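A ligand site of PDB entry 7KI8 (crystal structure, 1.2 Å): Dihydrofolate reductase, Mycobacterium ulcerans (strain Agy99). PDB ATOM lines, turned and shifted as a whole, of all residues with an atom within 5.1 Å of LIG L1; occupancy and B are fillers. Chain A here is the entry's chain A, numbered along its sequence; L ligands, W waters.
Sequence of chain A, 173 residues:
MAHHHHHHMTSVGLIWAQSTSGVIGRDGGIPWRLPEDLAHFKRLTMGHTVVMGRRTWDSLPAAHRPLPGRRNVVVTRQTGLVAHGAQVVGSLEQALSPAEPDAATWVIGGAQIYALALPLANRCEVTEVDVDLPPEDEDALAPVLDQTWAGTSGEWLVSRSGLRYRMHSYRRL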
ATOM      1  N   ILE A  15     -23.389  13.895 -19.628  1.00  0.00           N
ATOM      2  CA  ILE A  15     -24.309  14.264 -18.565  1.00  0.00           C
ATOM      3  C   ILE A  15     -23.478  14.762 -17.388  1.00  0.00           C
ATOM      4  O   ILE A  15     -22.489  14.106 -17.026  1.00  0.00           O
ATOM      5  CB  ILE A  15     -25.242  13.099 -18.190  1.00  0.00           C
ATOM      6  CG1 ILE A  15     -26.268  13.535 -17.133  1.00  0.00           C
ATOM      7  CG2 ILE A  15     -24.457  11.822 -17.783  1.00  0.00           C
ATOM      8  CD1 ILE A  15     -27.416  12.552 -16.944  1.00  0.00           C
ATOM      9  N   TRP A  16     -23.804  15.945 -16.866  1.00  0.00           N
ATOM     10  CA  TRP A  16     -23.090  16.512 -15.739  1.00  0.00           C
ATOM     11  C   TRP A  16     -24.006  17.417 -14.946  1.00  0.00           C
ATOM     12  O   TRP A  16     -25.032  17.870 -15.433  1.00  0.00           O
ATOM     13  CB  TRP A  16     -21.830  17.280 -16.167  1.00  0.00           C
ATOM     14  CG  TRP A  16     -22.000  18.623 -16.806  1.00  0.00           C
ATOM     15  CD1 TRP A  16     -22.120  19.822 -16.172  1.00  0.00           C
ATOM     16  CD2 TRP A  16     -21.929  18.927 -18.218  1.00  0.00           C
ATOM     17  NE1 TRP A  16     -22.156  20.838 -17.097  1.00  0.00           N
ATOM     18  CE2 TRP A  16     -22.048  20.321 -18.355  1.00  0.00           C
ATOM     19  CE3 TRP A  16     -21.786  18.144 -19.377  1.00  0.00           C
ATOM     20  CZ2 TRP A  16     -22.041  20.951 -19.593  1.00  0.00           C
ATOM     21  CZ3 TRP A  16     -21.787  18.773 -20.594  1.00  0.00           C
ATOM     22  CH2 TRP A  16     -21.908  20.163 -20.698  1.00  0.00           C
ATOM     23  N   ALA A  17     -23.598  17.686 -13.706  1.00  0.00           N
ATOM     24  CA  ALA A  17     -24.205  18.695 -12.846  1.00  0.00           C
ATOM     25  C   ALA A  17     -23.174  19.773 -12.545  1.00  0.00           C
ATOM     26  O   ALA A  17     -21.992  19.473 -12.311  1.00  0.00           O
ATOM     27  CB  ALA A  17     -24.712  18.069 -11.540  1.00  0.00           C
ATOM     28  N   ILE A  30     -17.771  16.193  -5.483  1.00  0.00           N
ATOM     29  CA  ILE A  30     -18.738  17.163  -5.978  1.00  0.00           C
ATOM     30  C   ILE A  30     -19.136  18.047  -4.803  1.00  0.00           C
ATOM     31  O   ILE A  30     -19.599  17.538  -3.775  1.00  0.00           O
ATOM     32  CB  ILE A  30     -19.953  16.474  -6.627  1.00  0.00           C
ATOM     33  CG1 ILE A  30     -19.515  15.651  -7.863  1.00  0.00           C
ATOM     34  CG2 ILE A  30     -21.011  17.493  -6.975  1.00  0.00           C
ATOM     35  CD1 ILE A  30     -20.636  14.862  -8.559  1.00  0.00           C
ATOM     36  N   ASP A  37     -30.928  15.588  -8.304  1.00  0.00           N
ATOM     37  CA  ASP A  37     -30.032  15.361  -9.436  1.00  0.00           C
ATOM     38  C   ASP A  37     -29.583  13.914  -9.508  1.00  0.00           C
ATOM     39  O   ASP A  37     -29.477  13.353 -10.604  1.00  0.00           O
ATOM     40  CB  ASP A  37     -28.820  16.284  -9.370  1.00  0.00           C
ATOM     41  CG  ASP A  37     -27.821  15.946 -10.450  1.00  0.00           C
ATOM     42  OD1 ASP A  37     -28.152  16.129 -11.644  1.00  0.00           O
ATOM     43  OD2 ASP A  37     -26.731  15.462 -10.097  1.00  0.00           O
ATOM     44  N   LEU A  38     -29.288  13.308  -8.356  1.00  0.00           N
ATOM     45  CA  LEU A  38     -28.913  11.896  -8.369  1.00  0.00           C
ATOM     46  C   LEU A  38     -30.010  11.045  -8.980  1.00  0.00           C
ATOM     47  O   LEU A  38     -29.732  10.140  -9.775  1.00  0.00           O
ATOM     48  CB  LEU A  38     -28.589  11.471  -6.938  1.00  0.00           C
ATOM     49  CG  LEU A  38     -28.061  10.084  -6.635  1.00  0.00           C
ATOM     50  CD1 LEU A  38     -27.282  10.163  -5.334  1.00  0.00           C
ATOM     51  CD2 LEU A  38     -29.200   9.089  -6.505  1.00  0.00           C
ATOM     52  N   HIS A  40     -32.322  12.008 -11.166  1.00  0.00           N
ATOM     53  CA  HIS A  40     -32.342  12.332 -12.590  1.00  0.00           C
ATOM     54  C   HIS A  40     -31.245  11.578 -13.318  1.00  0.00           C
ATOM     55  O   HIS A  40     -31.474  10.971 -14.374  1.00  0.00           O
ATOM     56  CB  HIS A  40     -32.159  13.844 -12.686  1.00  0.00           C
ATOM     57  CG  HIS A  40     -31.889  14.346 -14.069  1.00  0.00           C
ATOM     58  ND1 HIS A  40     -32.841  14.327 -15.061  1.00  0.00           N
ATOM     59  CD2 HIS A  40     -30.794  14.918 -14.610  1.00  0.00           C
ATOM     60  CE1 HIS A  40     -32.340  14.882 -16.154  1.00  0.00           C
ATOM     61  NE2 HIS A  40     -31.097  15.237 -15.910  1.00  0.00           N
ATOM     62  N   PHE A  41     -30.035  11.603 -12.767  1.00  0.00           N
ATOM     63  CA  PHE A  41     -28.895  10.899 -13.362  1.00  0.00           C
ATOM     64  C   PHE A  41     -29.168   9.402 -13.455  1.00  0.00           C
ATOM     65  O   PHE A  41     -28.924   8.768 -14.488  1.00  0.00           O
ATOM     66  CB  PHE A  41     -27.658  11.153 -12.516  1.00  0.00           C
ATOM     67  CG  PHE A  41     -26.464  10.364 -12.933  1.00  0.00           C
ATOM     68  CD1 PHE A  41     -25.661  10.799 -13.981  1.00  0.00           C
ATOM     69  CD2 PHE A  41     -26.165   9.164 -12.303  1.00  0.00           C
ATOM     70  CE1 PHE A  41     -24.560  10.057 -14.376  1.00  0.00           C
ATOM     71  CE2 PHE A  41     -25.051   8.428 -12.677  1.00  0.00           C
ATOM     72  CZ  PHE A  41     -24.256   8.856 -13.724  1.00  0.00           C
ATOM     73  N   LYS A  42     -29.718   8.821 -12.377  1.00  0.00           N
ATOM     74  CA  LYS A  42     -30.031   7.395 -12.369  1.00  0.00           C
ATOM     75  C   LYS A  42     -31.080   7.059 -13.430  1.00  0.00           C
ATOM     76  O   LYS A  42     -30.947   6.072 -14.164  1.00  0.00           O
ATOM     77  CB  LYS A  42     -30.485   7.010 -10.960  1.00  0.00           C
ATOM     78  CG  LYS A  42     -30.602   5.526 -10.659  1.00  0.00           C
ATOM     79  CD  LYS A  42     -31.099   5.301  -9.220  1.00  0.00           C
ATOM     80  CE  LYS A  42     -30.149   5.824  -8.141  1.00  0.00           C
ATOM     81  NZ  LYS A  42     -30.721   5.803  -6.742  1.00  0.00           N
ATOM     82  N   THR A  45     -29.513   7.143 -16.979  1.00  0.00           N
ATOM     83  CA  THR A  45     -28.411   6.232 -17.276  1.00  0.00           C
ATOM     84  C   THR A  45     -28.737   4.764 -17.033  1.00  0.00           C
ATOM     85  O   THR A  45     -28.000   3.909 -17.526  1.00  0.00           O
ATOM     86  CB  THR A  45     -27.134   6.605 -16.498  1.00  0.00           C
ATOM     87  OG1 THR A  45     -27.381   6.549 -15.092  1.00  0.00           O
ATOM     88  CG2 THR A  45     -26.574   7.989 -16.891  1.00  0.00           C
ATOM     89  N   THR A  56     -12.731  10.038 -11.694  1.00  0.00           N
ATOM     90  CA  THR A  56     -14.141   9.945 -11.306  1.00  0.00           C
ATOM     91  C   THR A  56     -14.449   8.562 -10.732  1.00  0.00           C
ATOM     92  O   THR A  56     -15.128   8.451  -9.709  1.00  0.00           O
ATOM     93  CB  THR A  56     -15.029  10.294 -12.510  1.00  0.00           C
ATOM     94  OG1 THR A  56     -14.841  11.678 -12.838  1.00  0.00           O
ATOM     95  CG2 THR A  56     -16.505  10.031 -12.238  1.00  0.00           C
ATOM     96  N   LEU A  60     -15.929   7.827  -6.639  1.00  0.00           N
ATOM     97  CA  LEU A  60     -17.240   7.337  -6.273  1.00  0.00           C
ATOM     98  C   LEU A  60     -17.222   6.806  -4.844  1.00  0.00           C
ATOM     99  O   LEU A  60     -16.283   6.086  -4.475  1.00  0.00           O
ATOM    100  CB  LEU A  60     -17.643   6.191  -7.194  1.00  0.00           C
ATOM    101  CG  LEU A  60     -17.939   6.619  -8.614  1.00  0.00           C
ATOM    102  CD1 LEU A  60     -18.039   5.391  -9.513  1.00  0.00           C
ATOM    103  CD2 LEU A  60     -19.236   7.402  -8.633  1.00  0.00           C
ATOM    104  N   PRO A  61     -18.220   7.131  -4.034  1.00  0.00           N
ATOM    105  CA  PRO A  61     -18.365   6.441  -2.741  1.00  0.00           C
ATOM    106  C   PRO A  61     -18.439   4.946  -2.971  1.00  0.00           C
ATOM    107  O   PRO A  61     -18.974   4.486  -3.987  1.00  0.00           O
ATOM    108  CB  PRO A  61     -19.687   6.997  -2.202  1.00  0.00           C
ATOM    109  CG  PRO A  61     -19.883   8.308  -2.895  1.00  0.00           C
ATOM    110  CD  PRO A  61     -19.285   8.115  -4.265  1.00  0.00           C
ATOM    111  N   HIS A  64     -21.364   2.968  -4.205  1.00  0.00           N
ATOM    112  CA  HIS A  64     -21.850   3.295  -5.539  1.00  0.00           C
ATOM    113  C   HIS A  64     -20.858   2.947  -6.626  1.00  0.00           C
ATOM    114  O   HIS A  64     -20.999   3.438  -7.753  1.00  0.00           O
ATOM    115  CB  HIS A  64     -22.142   4.792  -5.602  1.00  0.00           C
ATOM    116  CG  HIS A  64     -23.061   5.281  -4.535  1.00  0.00           C
ATOM    117  ND1 HIS A  64     -24.372   4.867  -4.437  1.00  0.00           N
ATOM    118  CD2 HIS A  64     -22.864   6.152  -3.514  1.00  0.00           C
ATOM    119  CE1 HIS A  64     -24.948   5.469  -3.410  1.00  0.00           C
ATOM    120  NE2 HIS A  64     -24.055   6.248  -2.829  1.00  0.00           N
ATOM    121  N   LEU A  67     -21.404   1.722 -10.510  1.00  0.00           N
ATOM    122  CA  LEU A  67     -22.773   2.186 -10.555  1.00  0.00           C
ATOM    123  C   LEU A  67     -23.677   1.003 -10.847  1.00  0.00           C
ATOM    124  O   LEU A  67     -23.524   0.371 -11.907  1.00  0.00           O
ATOM    125  CB  LEU A  67     -22.941   3.220 -11.661  1.00  0.00           C
ATOM    126  CG  LEU A  67     -22.634   4.663 -11.296  1.00  0.00           C
ATOM    127  CD1 LEU A  67     -21.198   4.817 -10.860  1.00  0.00           C
ATOM    128  CD2 LEU A  67     -22.940   5.590 -12.469  1.00  0.00           C
ATOM    129  N   PRO A  68     -24.605   0.642  -9.966  1.00  0.00           N
ATOM    130  CA  PRO A  68     -25.365  -0.589 -10.193  1.00  0.00           C
ATOM    131  C   PRO A  68     -26.306  -0.460 -11.369  1.00  0.00           C
ATOM    132  O   PRO A  68     -26.859   0.605 -11.632  1.00  0.00           O
ATOM    133  CB  PRO A  68     -26.138  -0.777  -8.886  1.00  0.00           C
ATOM    134  CG  PRO A  68     -26.186   0.552  -8.260  1.00  0.00           C
ATOM    135  CD  PRO A  68     -24.913   1.253  -8.665  1.00  0.00           C
ATOM    136  N   ARG A  70     -25.633  -0.585 -14.507  1.00  0.00           N
ATOM    137  CA  ARG A  70     -25.022   0.047 -15.651  1.00  0.00           C
ATOM    138  C   ARG A  70     -23.707  -0.632 -15.949  1.00  0.00           C
ATOM    139  O   ARG A  70     -23.050  -1.173 -15.053  1.00  0.00           O
ATOM    140  CB  ARG A  70     -24.816   1.526 -15.387  1.00  0.00           C
ATOM    141  CG  ARG A  70     -26.118   2.264 -15.592  1.00  0.00           C
ATOM    142  CD  ARG A  70     -26.276   3.409 -14.648  1.00  0.00           C
ATOM    143  NE  ARG A  70     -26.502   3.010 -13.265  1.00  0.00           N
ATOM    144  CZ  ARG A  70     -26.615   3.880 -12.270  1.00  0.00           C
ATOM    145  NH1 ARG A  70     -26.603   5.186 -12.487  1.00  0.00           N
ATOM    146  NH2 ARG A  70     -26.692   3.421 -11.018  1.00  0.00           N
ATOM    147  N   ILE A 108     -19.967  10.342 -18.211  1.00  0.00           N
ATOM    148  CA  ILE A 108     -20.431  10.820 -16.917  1.00  0.00           C
ATOM    149  C   ILE A 108     -19.364  11.570 -16.137  1.00  0.00           C
ATOM    150  O   ILE A 108     -19.548  11.836 -14.948  1.00  0.00           O
ATOM    151  CB  ILE A 108     -21.056   9.686 -16.083  1.00  0.00           C
ATOM    152  CG1 ILE A 108     -19.984   8.703 -15.599  1.00  0.00           C
ATOM    153  CG2 ILE A 108     -22.143   8.966 -16.884  1.00  0.00           C
ATOM    154  CD1 ILE A 108     -20.461   7.807 -14.456  1.00  0.00           C
ATOM    155  N   GLY A 109     -18.251  11.928 -16.786  1.00  0.00           N
ATOM    156  CA  GLY A 109     -17.216  12.779 -16.199  1.00  0.00           C
ATOM    157  C   GLY A 109     -15.879  12.081 -16.101  1.00  0.00           C
ATOM    158  O   GLY A 109     -15.757  10.894 -16.401  1.00  0.00           O
ATOM    159  N   TYR A 114     -14.816  14.647 -20.289  1.00  0.00           N
ATOM    160  CA  TYR A 114     -15.755  15.473 -21.040  1.00  0.00           C
ATOM    161  C   TYR A 114     -15.057  16.155 -22.207  1.00  0.00           C
ATOM    162  O   TYR A 114     -15.613  16.263 -23.304  1.00  0.00           O
ATOM    163  CB  TYR A 114     -16.412  16.552 -20.175  1.00  0.00           C
ATOM    164  CG  TYR A 114     -17.392  16.068 -19.130  1.00  0.00           C
ATOM    165  CD1 TYR A 114     -18.323  15.079 -19.423  1.00  0.00           C
ATOM    166  CD2 TYR A 114     -17.380  16.594 -17.858  1.00  0.00           C
ATOM    167  CE1 TYR A 114     -19.214  14.629 -18.448  1.00  0.00           C
ATOM    168  CE2 TYR A 114     -18.257  16.158 -16.887  1.00  0.00           C
ATOM    169  CZ  TYR A 114     -19.167  15.175 -17.182  1.00  0.00           C
ATOM    170  OH  TYR A 114     -20.003  14.718 -16.180  1.00  0.00           O
ATOM    171  N   THR A 127     -27.457  19.512 -15.339  1.00  0.00           N
ATOM    172  CA  THR A 127     -28.196  20.022 -14.196  1.00  0.00           C
ATOM    173  C   THR A 127     -27.452  21.240 -13.692  1.00  0.00           C
ATOM    174  O   THR A 127     -26.258  21.154 -13.391  1.00  0.00           O
ATOM    175  CB  THR A 127     -28.298  18.998 -13.076  1.00  0.00           C
ATOM    176  OG1 THR A 127     -28.900  17.816 -13.595  1.00  0.00           O
ATOM    177  CG2 THR A 127     -29.130  19.554 -11.911  1.00  0.00           C
HETATM  178  C1  LIG L   1     -21.547  10.433  -7.492  1.00  0.00           C
HETATM  179  C2  LIG L   1     -20.648  11.291  -6.873  1.00  0.00           C
HETATM  180  C3  LIG L   1     -20.715  11.525  -5.499  1.00  0.00           C
HETATM  181  C4  LIG L   1     -21.667  10.907  -4.725  1.00  0.00           C
HETATM  182  C5  LIG L   1     -22.581  10.055  -5.326  1.00  0.00           C
HETATM  183  C6  LIG L   1     -22.544   9.801  -6.674  1.00  0.00           C
HETATM  184  C7  LIG L   1     -25.415   8.608  -8.825  1.00  0.00           C
HETATM  185  C8  LIG L   1     -24.623   9.553  -7.924  1.00  0.00           C
HETATM  186  C9  LIG L   1     -26.353   6.282  -9.156  1.00  0.00           C
HETATM  187  C10 LIG L   1     -25.169  12.612  -9.303  1.00  0.00           C
HETATM  188  C11 LIG L   1     -23.892  13.316  -9.793  1.00  0.00           C
HETATM  189  C12 LIG L   1     -23.965  13.531 -11.279  1.00  0.00           C
HETATM  190  C13 LIG L   1     -25.167  14.423 -13.056  1.00  0.00           C
HETATM  191  C14 LIG L   1     -23.221  13.299 -13.534  1.00  0.00           C
HETATM  192  C15 LIG L   1     -23.036  13.041 -12.144  1.00  0.00           C
HETATM  193  C16 LIG L   1     -22.036  10.903 -11.739  1.00  0.00           C
HETATM  194  C17 LIG L   1     -20.716  10.358 -11.196  1.00  0.00           C
HETATM  195  C18 LIG L   1     -20.490  10.711  -9.709  1.00  0.00           C
HETATM  196  C19 LIG L   1     -23.875   7.749  -6.514  1.00  0.00           C
HETATM  197  C20 LIG L   1     -24.674   6.697  -7.286  1.00  0.00           C
HETATM  198  C21 LIG L   1     -25.816   7.322  -8.098  1.00  0.00           C
HETATM  199  N1  LIG L   1     -25.027  14.207 -11.746  1.00  0.00           N
HETATM  200  N2  LIG L   1     -26.264  15.082 -13.509  1.00  0.00           N
HETATM  201  N3  LIG L   1     -24.299  13.974 -13.960  1.00  0.00           N
HETATM  202  N4  LIG L   1     -22.316  12.880 -14.456  1.00  0.00           N
HETATM  203  N5  LIG L   1     -21.525  10.175  -8.850  1.00  0.00           N
HETATM  204  N6  LIG L   1     -23.455   8.930  -7.332  1.00  0.00           N
HETATM  205  O1  LIG L   1     -21.921  12.347 -11.753  1.00  0.00           O
HETATM  206  O2  LIG L   1     -26.579   5.123  -8.756  1.00  0.00           O
HETATM  207  O3  LIG L   1     -26.514   6.730 -10.301  1.00  0.00           O
HETATM  208  P1  LG2 L   2     -11.439  12.463 -14.886  1.00  0.00           P
HETATM  209  O1  LG2 L   2     -12.518  11.796 -14.134  1.00  0.00           O
HETATM  210  O2  LG2 L   2     -11.751  12.997 -16.258  1.00  0.00           O
HETATM  211  O3  LG2 L   2     -10.258  11.359 -14.969  1.00  0.00           O
HETATM  212  C1  LG2 L   2      -8.955  11.716 -15.470  1.00  0.00           C
HETATM  213  C2  LG2 L   2      -8.224  10.432 -15.749  1.00  0.00           C
HETATM  214  O4  LG2 L   2      -8.736   9.820 -16.955  1.00  0.00           O
HETATM  215  C3  LG2 L   2      -6.716  10.595 -15.986  1.00  0.00           C
HETATM  216  O5  LG2 L   2      -6.039  10.752 -14.748  1.00  0.00           O
HETATM  217  C4  LG2 L   2      -6.442   9.288 -16.734  1.00  0.00           C
HETATM  218  O6  LG2 L   2      -6.482   8.127 -15.871  1.00  0.00           O
HETATM  219  C5  LG2 L   2      -7.669   9.171 -17.635  1.00  0.00           C
HETATM  220  N1  LG2 L   2      -7.474   9.808 -18.929  1.00  0.00           N
HETATM  221  C6  LG2 L   2      -7.576  11.130 -19.262  1.00  0.00           C
HETATM  222  N2  LG2 L   2      -7.315  11.389 -20.524  1.00  0.00           N
HETATM  223  C7  LG2 L   2      -7.024  10.137 -21.057  1.00  0.00           C
HETATM  224  C8  LG2 L   2      -6.658   9.720 -22.355  1.00  0.00           C
HETATM  225  N3  LG2 L   2      -6.513  10.554 -23.390  1.00  0.00           N
HETATM  226  N4  LG2 L   2      -6.443   8.403 -22.545  1.00  0.00           N
HETATM  227  C9  LG2 L   2      -6.575   7.568 -21.509  1.00  0.00           C
HETATM  228  N5  LG2 L   2      -6.904   7.846 -20.248  1.00  0.00           N
HETATM  229  C10 LG2 L   2      -7.118   9.154 -20.087  1.00  0.00           C
HETATM  230  O7  LG2 L   2     -10.731  13.558 -13.986  1.00  0.00           O
HETATM  231  P2  LG2 L   2     -10.989  15.095 -13.650  1.00  0.00           P
HETATM  232  O8  LG2 L   2     -11.044  15.862 -14.905  1.00  0.00           O
HETATM  233  O9  LG2 L   2     -10.002  15.460 -12.621  1.00  0.00           O
HETATM  234  O10 LG2 L   2     -12.459  15.064 -13.053  1.00  0.00           O
HETATM  235  C11 LG2 L   2     -12.683  14.560 -11.719  1.00  0.00           C
HETATM  236  C12 LG2 L   2     -13.513  15.562 -10.943  1.00  0.00           C
HETATM  237  O11 LG2 L   2     -14.793  15.750 -11.598  1.00  0.00           O
HETATM  238  C13 LG2 L   2     -13.834  15.145  -9.506  1.00  0.00           C
HETATM  239  O12 LG2 L   2     -13.900  16.306  -8.689  1.00  0.00           O
HETATM  240  C14 LG2 L   2     -15.245  14.565  -9.653  1.00  0.00           C
HETATM  241  O13 LG2 L   2     -15.950  14.628  -8.415  1.00  0.00           O
HETATM  242  C15 LG2 L   2     -15.809  15.548 -10.648  1.00  0.00           C
HETATM  243  N6  LG2 L   2     -17.026  15.037 -11.366  1.00  0.00           N
HETATM  244  C16 LG2 L   2     -18.112  15.835 -11.368  1.00  0.00           C
HETATM  245  C17 LG2 L   2     -19.246  15.453 -12.051  1.00  0.00           C
HETATM  246  C18 LG2 L   2     -20.486  16.323 -12.074  1.00  0.00           C
HETATM  247  O14 LG2 L   2     -21.424  16.025 -12.826  1.00  0.00           O
HETATM  248  N7  LG2 L   2     -20.501  17.404 -11.291  1.00  0.00           N
HETATM  249  C19 LG2 L   2     -19.245  14.225 -12.713  1.00  0.00           C
HETATM  250  C20 LG2 L   2     -18.119  13.423 -12.675  1.00  0.00           C
HETATM  251  C21 LG2 L   2     -17.007  13.845 -11.986  1.00  0.00           C
HETATM  252  P3  LG2 L   2      -5.114   7.524 -15.296  1.00  0.00           P
HETATM  253  O15 LG2 L   2      -4.260   7.168 -16.462  1.00  0.00           O
HETATM  254  O16 LG2 L   2      -4.538   8.658 -14.447  1.00  0.00           O
HETATM  255  O17 LG2 L   2      -5.567   6.340 -14.511  1.00  0.00           O
HETATM  256  O   HOH W   1     -27.850  16.216 -15.755  1.00  0.00           O
HETATM  257  O   HOH W   2     -17.331  11.943  -5.163  1.00  0.00           O
HETATM  258  O   HOH W   3     -27.553   3.975  -6.714  1.00  0.00           O
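Trp 16 touches LIG L1 (CA to N3, 3.3 Å). Ala 17 touches LIG L1 (N to C13, 3.7 Å). CD1 of Ile 30 touches C11 of LIG L1 (3.8 Å). Leu 38 touches LIG L1. Phe 41 touches LIG L1 (CD2 to O3, 3.2 Å). Lys 42 touches LIG L1 (CE to O2, 3.7 Å). CD2 of Leu 60 touches N5 of LIG L1, 3.6 Å away. Pro 61 touches LIG L1 (CG to C4, 3.6 Å). His 64 touches LIG L1 (CG to C19, 3.3 Å). OG1 of Thr 127 touches N2 of LIG L1, at 3.8 Å. Hydrophobic or aromatic side chains that line LIG L1: Ile 15, Ala 17, Ile 30, Leu 38, Phe 41, Leu 60, Pro 61, His 64 and Ile 108. Within 4 Å of LIG L1: Ile 15, Trp 16, Ala 17, Ile 30, Asp 37, Leu 38, Phe 41, Lys 42, Leu 60, Pro 61, His 64, Arg 70, Ile 108, Tyr 114 and Thr 127.
The backbone carbonyl oxygen of Phe 41 lies within hydrogen-bond range of the side-chain hydroxyl of Thr 45, at 2.8 Å. The side-chain carboxylate (OD1) of Asp 37 lies within hydrogen-bond range of the side-chain hydroxyl (OG1) of Thr 127, 2.7 Å away. O of Ile 15 sits at hydrogen-bond distance from OH of Tyr 114, at 2.7 Å. The side-chain hydroxyl (OH) of Tyr 114 lies close to the backbone NH (N) of Gly 109, at 3.3 Å. The backbone carbonyl oxygen (O) of Trp 16 is in hydrogen-bond range of the backbone NH (N) of Thr 127, 2.9 Å away. The backbone carbonyl oxygen (O) of Pro 68 sits at hydrogen-bond distance from the guanidinium group (NH2) of Arg 70 (2.9 Å). OH of Tyr 114 sits at hydrogen-bond distance from O of Ile 108. The guanidinium group (NH1) of Arg 70 lies within hydrogen-bond range of the side-chain hydroxyl (OG1) of Thr 45 (3.0 Å).
O of Ile 108 is in hydrogen-bond range of N4 of LIG L1 (3.0 Å). OH of Tyr 114 is in hydrogen-bond range of N4 of LIG L1 (3.4 Å). An oxygen (O1) of LG2 L2 lies within hydrogen-bond range of the side-chain hydroxyl (OG1) of Thr 56. N of Ala 17 is in hydrogen-bond range of O14 of LG2 L2. O of Ile 15 lies within hydrogen-bond range of N4 of LIG L1. The guanidinium group (NH1) of Arg 70 lies within salt-bridge range of an oxygen (O3) of LIG L1. The backbone carbonyl oxygen (O) of Ala 17 sits at hydrogen-bond distance from a nitrogen (N7) of LG2 L2. OD2 of Asp 37 sits at hydrogen-bond distance from N1 of LIG L1, 2.7 Å away. The backbone NH of Thr 56 sits at hydrogen-bond distance from an oxygen (O1) of LG2 L2 (3.0 Å).
Water W1 lies within hydrogen-bond range of OG1 of Thr 127 (2.9 Å), N2 of LIG L1 (3.0 Å), O of Trp 16 (3.3 Å) and NE2 of His 40 (3.4 Å).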
